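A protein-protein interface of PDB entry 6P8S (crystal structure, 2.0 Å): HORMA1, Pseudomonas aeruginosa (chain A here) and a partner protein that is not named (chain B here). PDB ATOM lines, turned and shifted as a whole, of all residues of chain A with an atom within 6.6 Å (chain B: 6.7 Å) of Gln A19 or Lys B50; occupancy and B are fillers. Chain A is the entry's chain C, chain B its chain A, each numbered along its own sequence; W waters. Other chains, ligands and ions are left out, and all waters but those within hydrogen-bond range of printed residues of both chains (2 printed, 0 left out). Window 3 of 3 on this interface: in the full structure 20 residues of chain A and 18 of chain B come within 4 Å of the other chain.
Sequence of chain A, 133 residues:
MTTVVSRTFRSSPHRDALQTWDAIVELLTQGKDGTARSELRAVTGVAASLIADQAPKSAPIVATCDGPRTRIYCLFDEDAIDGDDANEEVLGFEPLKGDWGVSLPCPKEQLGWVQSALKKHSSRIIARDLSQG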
ATOM      1  N   PRO A  13      -5.876   8.332  12.389  1.00  0.00           N
ATOM      2  CA  PRO A  13      -7.093   9.129  12.585  1.00  0.00           C
ATOM      3  C   PRO A  13      -8.421   8.436  12.280  1.00  0.00           C
ATOM      4  O   PRO A  13      -9.457   9.105  12.325  1.00  0.00           O
ATOM      5  CB  PRO A  13      -6.888  10.294  11.599  1.00  0.00           C
ATOM      6  CG  PRO A  13      -6.199   9.602  10.427  1.00  0.00           C
ATOM      7  CD  PRO A  13      -5.317   8.512  11.036  1.00  0.00           C
ATOM      8  N   HIS A  14      -8.402   7.138  11.971  1.00  0.00           N
ATOM      9  CA  HIS A  14      -9.655   6.417  11.767  1.00  0.00           C
ATOM     10  C   HIS A  14     -10.458   6.366  13.057  1.00  0.00           C
ATOM     11  O   HIS A  14     -11.660   6.659  13.071  1.00  0.00           O
ATOM     12  CB  HIS A  14      -9.368   5.006  11.260  1.00  0.00           C
ATOM     13  CG  HIS A  14     -10.585   4.151  11.136  1.00  0.00           C
ATOM     14  ND1 HIS A  14     -11.519   4.338  10.142  1.00  0.00           N
ATOM     15  CD2 HIS A  14     -11.019   3.099  11.871  1.00  0.00           C
ATOM     16  CE1 HIS A  14     -12.477   3.436  10.268  1.00  0.00           C
ATOM     17  NE2 HIS A  14     -12.202   2.679  11.315  1.00  0.00           N
ATOM     18  N   ARG A  15      -9.813   5.952  14.144  1.00  0.00           N
ATOM     19  CA  ARG A  15     -10.351   6.026  15.493  1.00  0.00           C
ATOM     20  C   ARG A  15      -9.449   6.925  16.336  1.00  0.00           C
ATOM     21  O   ARG A  15      -8.220   6.921  16.155  1.00  0.00           O
ATOM     22  CB  ARG A  15     -10.408   4.660  16.142  1.00  0.00           C
ATOM     23  CG  ARG A  15     -11.524   3.733  15.669  1.00  0.00           C
ATOM     24  CD  ARG A  15     -11.423   2.447  16.487  1.00  0.00           C
ATOM     25  NE  ARG A  15     -12.321   1.400  16.039  1.00  0.00           N
ATOM     26  CZ  ARG A  15     -11.950   0.366  15.287  1.00  0.00           C
ATOM     27  NH1 ARG A  15     -10.686   0.233  14.882  1.00  0.00           N
ATOM     28  NH2 ARG A  15     -12.851  -0.542  14.949  1.00  0.00           N
ATOM     29  N   ASP A  16     -10.032   7.666  17.280  1.00  0.00           N
ATOM     30  CA  ASP A  16      -9.179   8.363  18.229  1.00  0.00           C
ATOM     31  C   ASP A  16      -8.655   7.360  19.258  1.00  0.00           C
ATOM     32  O   ASP A  16      -9.121   6.216  19.357  1.00  0.00           O
ATOM     33  CB  ASP A  16      -9.908   9.529  18.894  1.00  0.00           C
ATOM     34  CG  ASP A  16     -11.109   9.094  19.720  1.00  0.00           C
ATOM     35  OD1 ASP A  16     -10.948   8.240  20.614  1.00  0.00           O
ATOM     36  OD2 ASP A  16     -12.207   9.642  19.489  1.00  0.00           O
ATOM     37  N   ALA A  17      -7.644   7.792  20.012  1.00  0.00           N
ATOM     38  CA  ALA A  17      -6.958   6.884  20.926  1.00  0.00           C
ATOM     39  C   ALA A  17      -7.922   6.284  21.939  1.00  0.00           C
ATOM     40  O   ALA A  17      -7.819   5.095  22.273  1.00  0.00           O
ATOM     41  CB  ALA A  17      -5.807   7.615  21.631  1.00  0.00           C
ATOM     42  N   LEU A  18      -8.868   7.087  22.435  1.00  0.00           N
ATOM     43  CA  LEU A  18      -9.888   6.568  23.344  1.00  0.00           C
ATOM     44  C   LEU A  18     -10.708   5.475  22.671  1.00  0.00           C
ATOM     45  O   LEU A  18     -10.908   4.387  23.228  1.00  0.00           O
ATOM     46  CB  LEU A  18     -10.799   7.702  23.798  1.00  0.00           C
ATOM     47  CG  LEU A  18     -12.009   7.315  24.637  1.00  0.00           C
ATOM     48  CD1 LEU A  18     -11.616   6.788  25.989  1.00  0.00           C
ATOM     49  CD2 LEU A  18     -12.943   8.527  24.767  1.00  0.00           C
ATOM     50  N   GLN A  19     -11.220   5.761  21.475  1.00  0.00           N
ATOM     51  CA  GLN A  19     -11.996   4.767  20.742  1.00  0.00           C
ATOM     52  C   GLN A  19     -11.174   3.513  20.457  1.00  0.00           C
ATOM     53  O   GLN A  19     -11.691   2.388  20.537  1.00  0.00           O
ATOM     54  CB  GLN A  19     -12.511   5.374  19.438  1.00  0.00           C
ATOM     55  CG  GLN A  19     -13.493   6.507  19.628  1.00  0.00           C
ATOM     56  CD  GLN A  19     -13.913   7.127  18.312  1.00  0.00           C
ATOM     57  OE1 GLN A  19     -13.137   7.172  17.358  1.00  0.00           O
ATOM     58  NE2 GLN A  19     -15.145   7.604  18.251  1.00  0.00           N
ATOM     59  N   THR A  20      -9.897   3.688  20.111  1.00  0.00           N
ATOM     60  CA  THR A  20      -9.034   2.546  19.834  1.00  0.00           C
ATOM     61  C   THR A  20      -8.979   1.601  21.031  1.00  0.00           C
ATOM     62  O   THR A  20      -9.113   0.378  20.889  1.00  0.00           O
ATOM     63  CB  THR A  20      -7.624   3.024  19.456  1.00  0.00           C
ATOM     64  OG1 THR A  20      -7.681   3.895  18.315  1.00  0.00           O
ATOM     65  CG2 THR A  20      -6.750   1.830  19.124  1.00  0.00           C
ATOM     66  N   TRP A  21      -8.782   2.150  22.226  1.00  0.00           N
ATOM     67  CA  TRP A  21      -8.693   1.300  23.411  1.00  0.00           C
ATOM     68  C   TRP A  21     -10.021   0.616  23.722  1.00  0.00           C
ATOM     69  O   TRP A  21     -10.046  -0.544  24.158  1.00  0.00           O
ATOM     70  CB  TRP A  21      -8.255   2.121  24.613  1.00  0.00           C
ATOM     71  CG  TRP A  21      -8.220   1.334  25.882  1.00  0.00           C
ATOM     72  CD1 TRP A  21      -8.991   1.530  26.990  1.00  0.00           C
ATOM     73  CD2 TRP A  21      -7.362   0.231  26.178  1.00  0.00           C
ATOM     74  NE1 TRP A  21      -8.658   0.618  27.962  1.00  0.00           N
ATOM     75  CE2 TRP A  21      -7.656  -0.187  27.485  1.00  0.00           C
ATOM     76  CE3 TRP A  21      -6.367  -0.437  25.470  1.00  0.00           C
ATOM     77  CZ2 TRP A  21      -6.993  -1.246  28.094  1.00  0.00           C
ATOM     78  CZ3 TRP A  21      -5.714  -1.492  26.075  1.00  0.00           C
ATOM     79  CH2 TRP A  21      -6.026  -1.881  27.374  1.00  0.00           C
ATOM     80  N   ASP A  22     -11.137   1.318  23.541  1.00  0.00           N
ATOM     81  CA  ASP A  22     -12.428   0.688  23.807  1.00  0.00           C
ATOM     82  C   ASP A  22     -12.663  -0.482  22.857  1.00  0.00           C
ATOM     83  O   ASP A  22     -13.201  -1.523  23.258  1.00  0.00           O
ATOM     84  CB  ASP A  22     -13.556   1.706  23.686  1.00  0.00           C
ATOM     85  CG  ASP A  22     -14.908   1.136  24.124  1.00  0.00           C
ATOM     86  OD1 ASP A  22     -15.086   0.830  25.328  1.00  0.00           O
ATOM     87  OD2 ASP A  22     -15.801   0.991  23.261  1.00  0.00           O
ATOM     88  N   ALA A  23     -12.254  -0.332  21.590  1.00  0.00           N
ATOM     89  CA  ALA A  23     -12.347  -1.438  20.640  1.00  0.00           C
ATOM     90  C   ALA A  23     -11.498  -2.614  21.094  1.00  0.00           C
ATOM     91  O   ALA A  23     -11.912  -3.769  20.966  1.00  0.00           O
ATOM     92  CB  ALA A  23     -11.921  -0.980  19.245  1.00  0.00           C
ATOM     93  N   ILE A  24     -10.306  -2.339  21.636  1.00  0.00           N
ATOM     94  CA  ILE A  24      -9.448  -3.409  22.135  1.00  0.00           C
ATOM     95  C   ILE A  24     -10.044  -4.032  23.393  1.00  0.00           C
ATOM     96  O   ILE A  24      -9.978  -5.255  23.584  1.00  0.00           O
ATOM     97  CB  ILE A  24      -8.023  -2.879  22.372  1.00  0.00           C
ATOM     98  CG1 ILE A  24      -7.401  -2.462  21.036  1.00  0.00           C
ATOM     99  CG2 ILE A  24      -7.159  -3.932  23.056  1.00  0.00           C
ATOM    100  CD1 ILE A  24      -6.025  -1.834  21.150  1.00  0.00           C
ATOM    101  N   ALA A  48      -4.924   4.953  26.384  1.00  0.00           N
ATOM    102  CA  ALA A  48      -5.151   5.893  25.289  1.00  0.00           C
ATOM    103  C   ALA A  48      -3.948   6.802  25.096  1.00  0.00           C
ATOM    104  O   ALA A  48      -3.556   7.101  23.962  1.00  0.00           O
ATOM    105  CB  ALA A  48      -6.410   6.722  25.559  1.00  0.00           C
ATOM    106  N   THR B  10     -13.543  14.574   9.528  1.00  0.00           N
ATOM    107  CA  THR B  10     -13.477  13.854  10.798  1.00  0.00           C
ATOM    108  C   THR B  10     -12.107  13.225  11.008  1.00  0.00           C
ATOM    109  O   THR B  10     -11.650  13.103  12.151  1.00  0.00           O
ATOM    110  CB  THR B  10     -14.569  12.782  10.860  1.00  0.00           C
ATOM    111  OG1 THR B  10     -15.852  13.409  10.705  1.00  0.00           O
ATOM    112  CG2 THR B  10     -14.516  12.044  12.197  1.00  0.00           C
ATOM    113  N   VAL B  13     -10.073  16.118  12.204  1.00  0.00           N
ATOM    114  CA  VAL B  13     -10.466  16.382  13.587  1.00  0.00           C
ATOM    115  C   VAL B  13      -9.797  15.385  14.526  1.00  0.00           C
ATOM    116  O   VAL B  13      -9.213  15.758  15.556  1.00  0.00           O
ATOM    117  CB  VAL B  13     -12.000  16.341  13.719  1.00  0.00           C
ATOM    118  CG1 VAL B  13     -12.428  16.359  15.183  1.00  0.00           C
ATOM    119  CG2 VAL B  13     -12.629  17.507  12.964  1.00  0.00           C
ATOM    120  N   THR B  14      -9.877  14.101  14.187  1.00  0.00           N
ATOM    121  CA  THR B  14      -9.335  13.067  15.057  1.00  0.00           C
ATOM    122  C   THR B  14      -7.831  13.226  15.220  1.00  0.00           C
ATOM    123  O   THR B  14      -7.298  13.084  16.327  1.00  0.00           O
ATOM    124  CB  THR B  14      -9.666  11.688  14.486  1.00  0.00           C
ATOM    125  OG1 THR B  14     -11.087  11.530  14.417  1.00  0.00           O
ATOM    126  CG2 THR B  14      -9.059  10.602  15.347  1.00  0.00           C
ATOM    127  N   THR B  17      -7.139  16.149  17.528  1.00  0.00           N
ATOM    128  CA  THR B  17      -7.542  15.857  18.899  1.00  0.00           C
ATOM    129  C   THR B  17      -6.485  15.012  19.600  1.00  0.00           C
ATOM    130  O   THR B  17      -5.960  15.393  20.654  1.00  0.00           O
ATOM    131  CB  THR B  17      -8.890  15.130  18.907  1.00  0.00           C
ATOM    132  OG1 THR B  17      -9.900  15.963  18.319  1.00  0.00           O
ATOM    133  CG2 THR B  17      -9.304  14.772  20.334  1.00  0.00           C
ATOM    134  N   ASN B  45     -11.688  14.769  28.150  1.00  0.00           N
ATOM    135  CA  ASN B  45     -11.031  15.763  27.305  1.00  0.00           C
ATOM    136  C   ASN B  45     -11.173  15.419  25.828  1.00  0.00           C
ATOM    137  O   ASN B  45     -11.430  16.304  25.000  1.00  0.00           O
ATOM    138  CB  ASN B  45      -9.556  15.889  27.697  1.00  0.00           C
ATOM    139  CG  ASN B  45      -9.376  16.507  29.071  1.00  0.00           C
ATOM    140  OD1 ASN B  45     -10.309  17.086  29.629  1.00  0.00           O
ATOM    141  ND2 ASN B  45      -8.171  16.395  29.619  1.00  0.00           N
ATOM    142  N   THR B  46     -10.999  14.138  25.474  1.00  0.00           N
ATOM    143  CA  THR B  46     -11.169  13.723  24.086  1.00  0.00           C
ATOM    144  C   THR B  46     -12.558  14.089  23.573  1.00  0.00           C
ATOM    145  O   THR B  46     -12.699  14.778  22.562  1.00  0.00           O
ATOM    146  CB  THR B  46     -10.935  12.216  23.958  1.00  0.00           C
ATOM    147  OG1 THR B  46      -9.557  11.914  24.208  1.00  0.00           O
ATOM    148  CG2 THR B  46     -11.326  11.724  22.564  1.00  0.00           C
ATOM    149  N   ARG B  47     -13.603  13.660  24.278  1.00  0.00           N
ATOM    150  CA  ARG B  47     -14.958  13.850  23.769  1.00  0.00           C
ATOM    151  C   ARG B  47     -15.288  15.326  23.593  1.00  0.00           C
ATOM    152  O   ARG B  47     -15.897  15.718  22.590  1.00  0.00           O
ATOM    153  CB  ARG B  47     -15.958  13.161  24.697  1.00  0.00           C
ATOM    154  CG  ARG B  47     -15.739  11.641  24.744  1.00  0.00           C
ATOM    155  CD  ARG B  47     -16.981  10.839  25.140  1.00  0.00           C
ATOM    156  NE  ARG B  47     -16.733   9.411  24.915  1.00  0.00           N
ATOM    157  CZ  ARG B  47     -16.636   8.492  25.877  1.00  0.00           C
ATOM    158  NH1 ARG B  47     -16.786   8.830  27.151  1.00  0.00           N
ATOM    159  NH2 ARG B  47     -16.397   7.224  25.562  1.00  0.00           N
ATOM    160  N   ALA B  48     -14.865  16.167  24.533  1.00  0.00           N
ATOM    161  CA  ALA B  48     -15.136  17.597  24.417  1.00  0.00           C
ATOM    162  C   ALA B  48     -14.387  18.209  23.240  1.00  0.00           C
ATOM    163  O   ALA B  48     -14.977  18.931  22.425  1.00  0.00           O
ATOM    164  CB  ALA B  48     -14.759  18.312  25.718  1.00  0.00           C
ATOM    165  N   ILE B  49     -13.081  17.937  23.140  1.00  0.00           N
ATOM    166  CA  ILE B  49     -12.272  18.524  22.074  1.00  0.00           C
ATOM    167  C   ILE B  49     -12.748  18.043  20.706  1.00  0.00           C
ATOM    168  O   ILE B  49     -12.937  18.837  19.774  1.00  0.00           O
ATOM    169  CB  ILE B  49     -10.789  18.187  22.293  1.00  0.00           C
ATOM    170  CG1 ILE B  49     -10.270  18.885  23.545  1.00  0.00           C
ATOM    171  CG2 ILE B  49      -9.961  18.598  21.077  1.00  0.00           C
ATOM    172  CD1 ILE B  49      -8.920  18.405  24.006  1.00  0.00           C
ATOM    173  N   LYS B  50     -12.938  16.730  20.562  1.00  0.00           N
ATOM    174  CA  LYS B  50     -13.377  16.191  19.279  1.00  0.00           C
ATOM    175  C   LYS B  50     -14.718  16.773  18.866  1.00  0.00           C
ATOM    176  O   LYS B  50     -14.928  17.092  17.690  1.00  0.00           O
ATOM    177  CB  LYS B  50     -13.460  14.672  19.352  1.00  0.00           C
ATOM    178  CG  LYS B  50     -13.584  13.997  18.005  1.00  0.00           C
ATOM    179  CD  LYS B  50     -13.067  12.572  18.094  1.00  0.00           C
ATOM    180  CE  LYS B  50     -13.340  11.797  16.829  1.00  0.00           C
ATOM    181  NZ  LYS B  50     -13.446  10.348  17.156  1.00  0.00           N
ATOM    182  N   THR B  51     -15.637  16.921  19.821  1.00  0.00           N
ATOM    183  CA  THR B  51     -16.958  17.449  19.504  1.00  0.00           C
ATOM    184  C   THR B  51     -16.858  18.878  18.987  1.00  0.00           C
ATOM    185  O   THR B  51     -17.397  19.207  17.924  1.00  0.00           O
ATOM    186  CB  THR B  51     -17.858  17.390  20.742  1.00  0.00           C
ATOM    187  OG1 THR B  51     -18.022  16.032  21.152  1.00  0.00           O
ATOM    188  CG2 THR B  51     -19.218  18.001  20.452  1.00  0.00           C
ATOM    189  N   TRP B  52     -16.181  19.749  19.738  1.00  0.00           N
ATOM    190  CA  TRP B  52     -16.143  21.169  19.406  1.00  0.00           C
ATOM    191  C   TRP B  52     -15.202  21.484  18.254  1.00  0.00           C
ATOM    192  O   TRP B  52     -15.431  22.476  17.561  1.00  0.00           O
ATOM    193  CB  TRP B  52     -15.793  21.960  20.671  1.00  0.00           C
ATOM    194  CG  TRP B  52     -16.976  21.954  21.661  1.00  0.00           C
ATOM    195  CD1 TRP B  52     -18.308  21.912  21.342  1.00  0.00           C
ATOM    196  CD2 TRP B  52     -16.918  21.986  23.097  1.00  0.00           C
ATOM    197  NE1 TRP B  52     -19.074  21.920  22.480  1.00  0.00           N
ATOM    198  CE2 TRP B  52     -18.247  21.965  23.572  1.00  0.00           C
ATOM    199  CE3 TRP B  52     -15.874  22.034  24.021  1.00  0.00           C
ATOM    200  CZ2 TRP B  52     -18.554  21.990  24.935  1.00  0.00           C
ATOM    201  CZ3 TRP B  52     -16.170  22.056  25.360  1.00  0.00           C
ATOM    202  CH2 TRP B  52     -17.502  22.040  25.812  1.00  0.00           C
ATOM    203  N   LEU B  53     -14.189  20.651  17.998  1.00  0.00           N
ATOM    204  CA  LEU B  53     -13.488  20.746  16.723  1.00  0.00           C
ATOM    205  C   LEU B  53     -14.414  20.366  15.573  1.00  0.00           C
ATOM    206  O   LEU B  53     -14.445  21.042  14.542  1.00  0.00           O
ATOM    207  CB  LEU B  53     -12.262  19.849  16.730  1.00  0.00           C
ATOM    208  CG  LEU B  53     -10.970  20.349  17.358  1.00  0.00           C
ATOM    209  CD1 LEU B  53      -9.893  19.257  17.212  1.00  0.00           C
ATOM    210  CD2 LEU B  53     -10.495  21.653  16.746  1.00  0.00           C
ATOM    211  N   GLY B  54     -15.209  19.304  15.749  1.00  0.00           N
ATOM    212  CA  GLY B  54     -16.089  18.861  14.679  1.00  0.00           C
ATOM    213  C   GLY B  54     -17.092  19.918  14.268  1.00  0.00           C
ATOM    214  O   GLY B  54     -17.420  20.050  13.085  1.00  0.00           O
ATOM    215  N   THR B  55     -17.594  20.687  15.235  1.00  0.00           N
ATOM    216  CA  THR B  55     -18.577  21.723  14.946  1.00  0.00           C
ATOM    217  C   THR B  55     -17.941  23.070  14.636  1.00  0.00           C
ATOM    218  O   THR B  55     -18.658  24.016  14.286  1.00  0.00           O
ATOM    219  CB  THR B  55     -19.542  21.901  16.131  1.00  0.00           C
ATOM    220  OG1 THR B  55     -18.820  22.377  17.272  1.00  0.00           O
ATOM    221  CG2 THR B  55     -20.216  20.587  16.487  1.00  0.00           C
ATOM    222  N   LEU B  58     -14.555  25.073  18.806  1.00  0.00           N
ATOM    223  CA  LEU B  58     -13.391  25.151  19.681  1.00  0.00           C
ATOM    224  C   LEU B  58     -12.462  26.274  19.220  1.00  0.00           C
ATOM    225  O   LEU B  58     -12.008  26.285  18.070  1.00  0.00           O
ATOM    226  CB  LEU B  58     -12.657  23.813  19.710  1.00  0.00           C
ATOM    227  CG  LEU B  58     -11.511  23.749  20.723  1.00  0.00           C
ATOM    228  CD1 LEU B  58     -12.019  23.934  22.146  1.00  0.00           C
ATOM    229  CD2 LEU B  58     -10.744  22.450  20.618  1.00  0.00           C
HETATM  230  O   HOH W   1     -12.709   9.203  14.558  1.00  0.00           O
HETATM  231  O   HOH W   2      -8.228  10.227  22.381  1.00  0.00           O
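Water W2 lies within hydrogen-bond range of OG1 of Thr B46 (2.8 Å), N of Leu A18 (3.2 Å) and N of Ala A17 (3.4 Å).
Water W1 lies within hydrogen-bond range of OG1 of Thr B14 (2.8 Å), NZ of Lys B50 (2.9 Å), O of His A14 (3.1 Å) and OE1 of Gln A19 (3.5 Å).
The side-chain amino group of Lys B50 lies within salt-bridge range of the side-chain carboxylate of Asp A16 (2.7 Å).
NZ of Lys B50 lies within hydrogen-bond range of OE1 of Gln A19.
Pro A13 touches Thr B14.
C of Arg A15 touches CG2 of Thr B14 (3.8 Å).
Asp A16 touches Thr B14.
Thr B46 touches Asp A16 (CG2 to OD2, 3.8 Å).
Leu A18 touches Arg B47 (CD2 to NH2, 3.8 Å).
The side-chain hydroxyl (OG1) of Thr A20 sits at hydrogen-bond distance from the backbone carbonyl oxygen (O) of Asp A16.
The side-chain hydroxyl of Thr B14 is in hydrogen-bond range of the backbone carbonyl oxygen of Thr B10, 2.8 Å away.
The side-chain carboxylate (OD1) of Asp A16 is in hydrogen-bond range of the backbone NH (N) of Leu A18, at 3.0 Å.
The backbone carbonyl oxygen (O) of Arg B47 is in hydrogen-bond range of the side-chain hydroxyl (OG1) of Thr B51, at 2.6 Å.
The backbone NH of Gln A19 lies within hydrogen-bond range of the side-chain carboxylate of Asp A16.
Of the 13 printed residues of chain A, 5 touch a printed residue of chain B.
Printed residues of chain A that touch a printed residue of chain B: Pro A13, Arg A15, Asp A16, Leu A18 and Gln A19.
Among the printed residues, 7 pairs touch across the chains.
Among the printed residues, Asp or Glu carboxylates within 4 Å of a Lys or Arg side-chain nitrogen of the other chain: Asp A16 with Lys B50 (2.7 Å).
Gln A19 touches one residue of chain B.
Of the printed residues of chain B, Pro A13 touches Thr B14.
Printed residues of chain B within 4 Å of Asp A16: Thr B14 (3.6 Å), Thr B46 (3.8 Å) and Lys B50 (2.7 Å).
Of the printed residues of chain A, Arg B47 touches Leu A18 (3.8 Å).
Printed residues of chain A within 4 Å of Thr B46: Asp A16 (3.8 Å).
Of the printed residues of chain A, Thr B14 touches Pro A13, Arg A15 and Asp A16.
Ala B48 touches none of the printed residues of chain A.
Trp B52 touches none of the printed residues of chain A.
The nearest residue of chain A that does not touch Lys B50 is Arg A15 (5.3 Å).
The nearest printed residue of chain B that does not touch Pro A13 is Thr B10 (4.6 Å).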
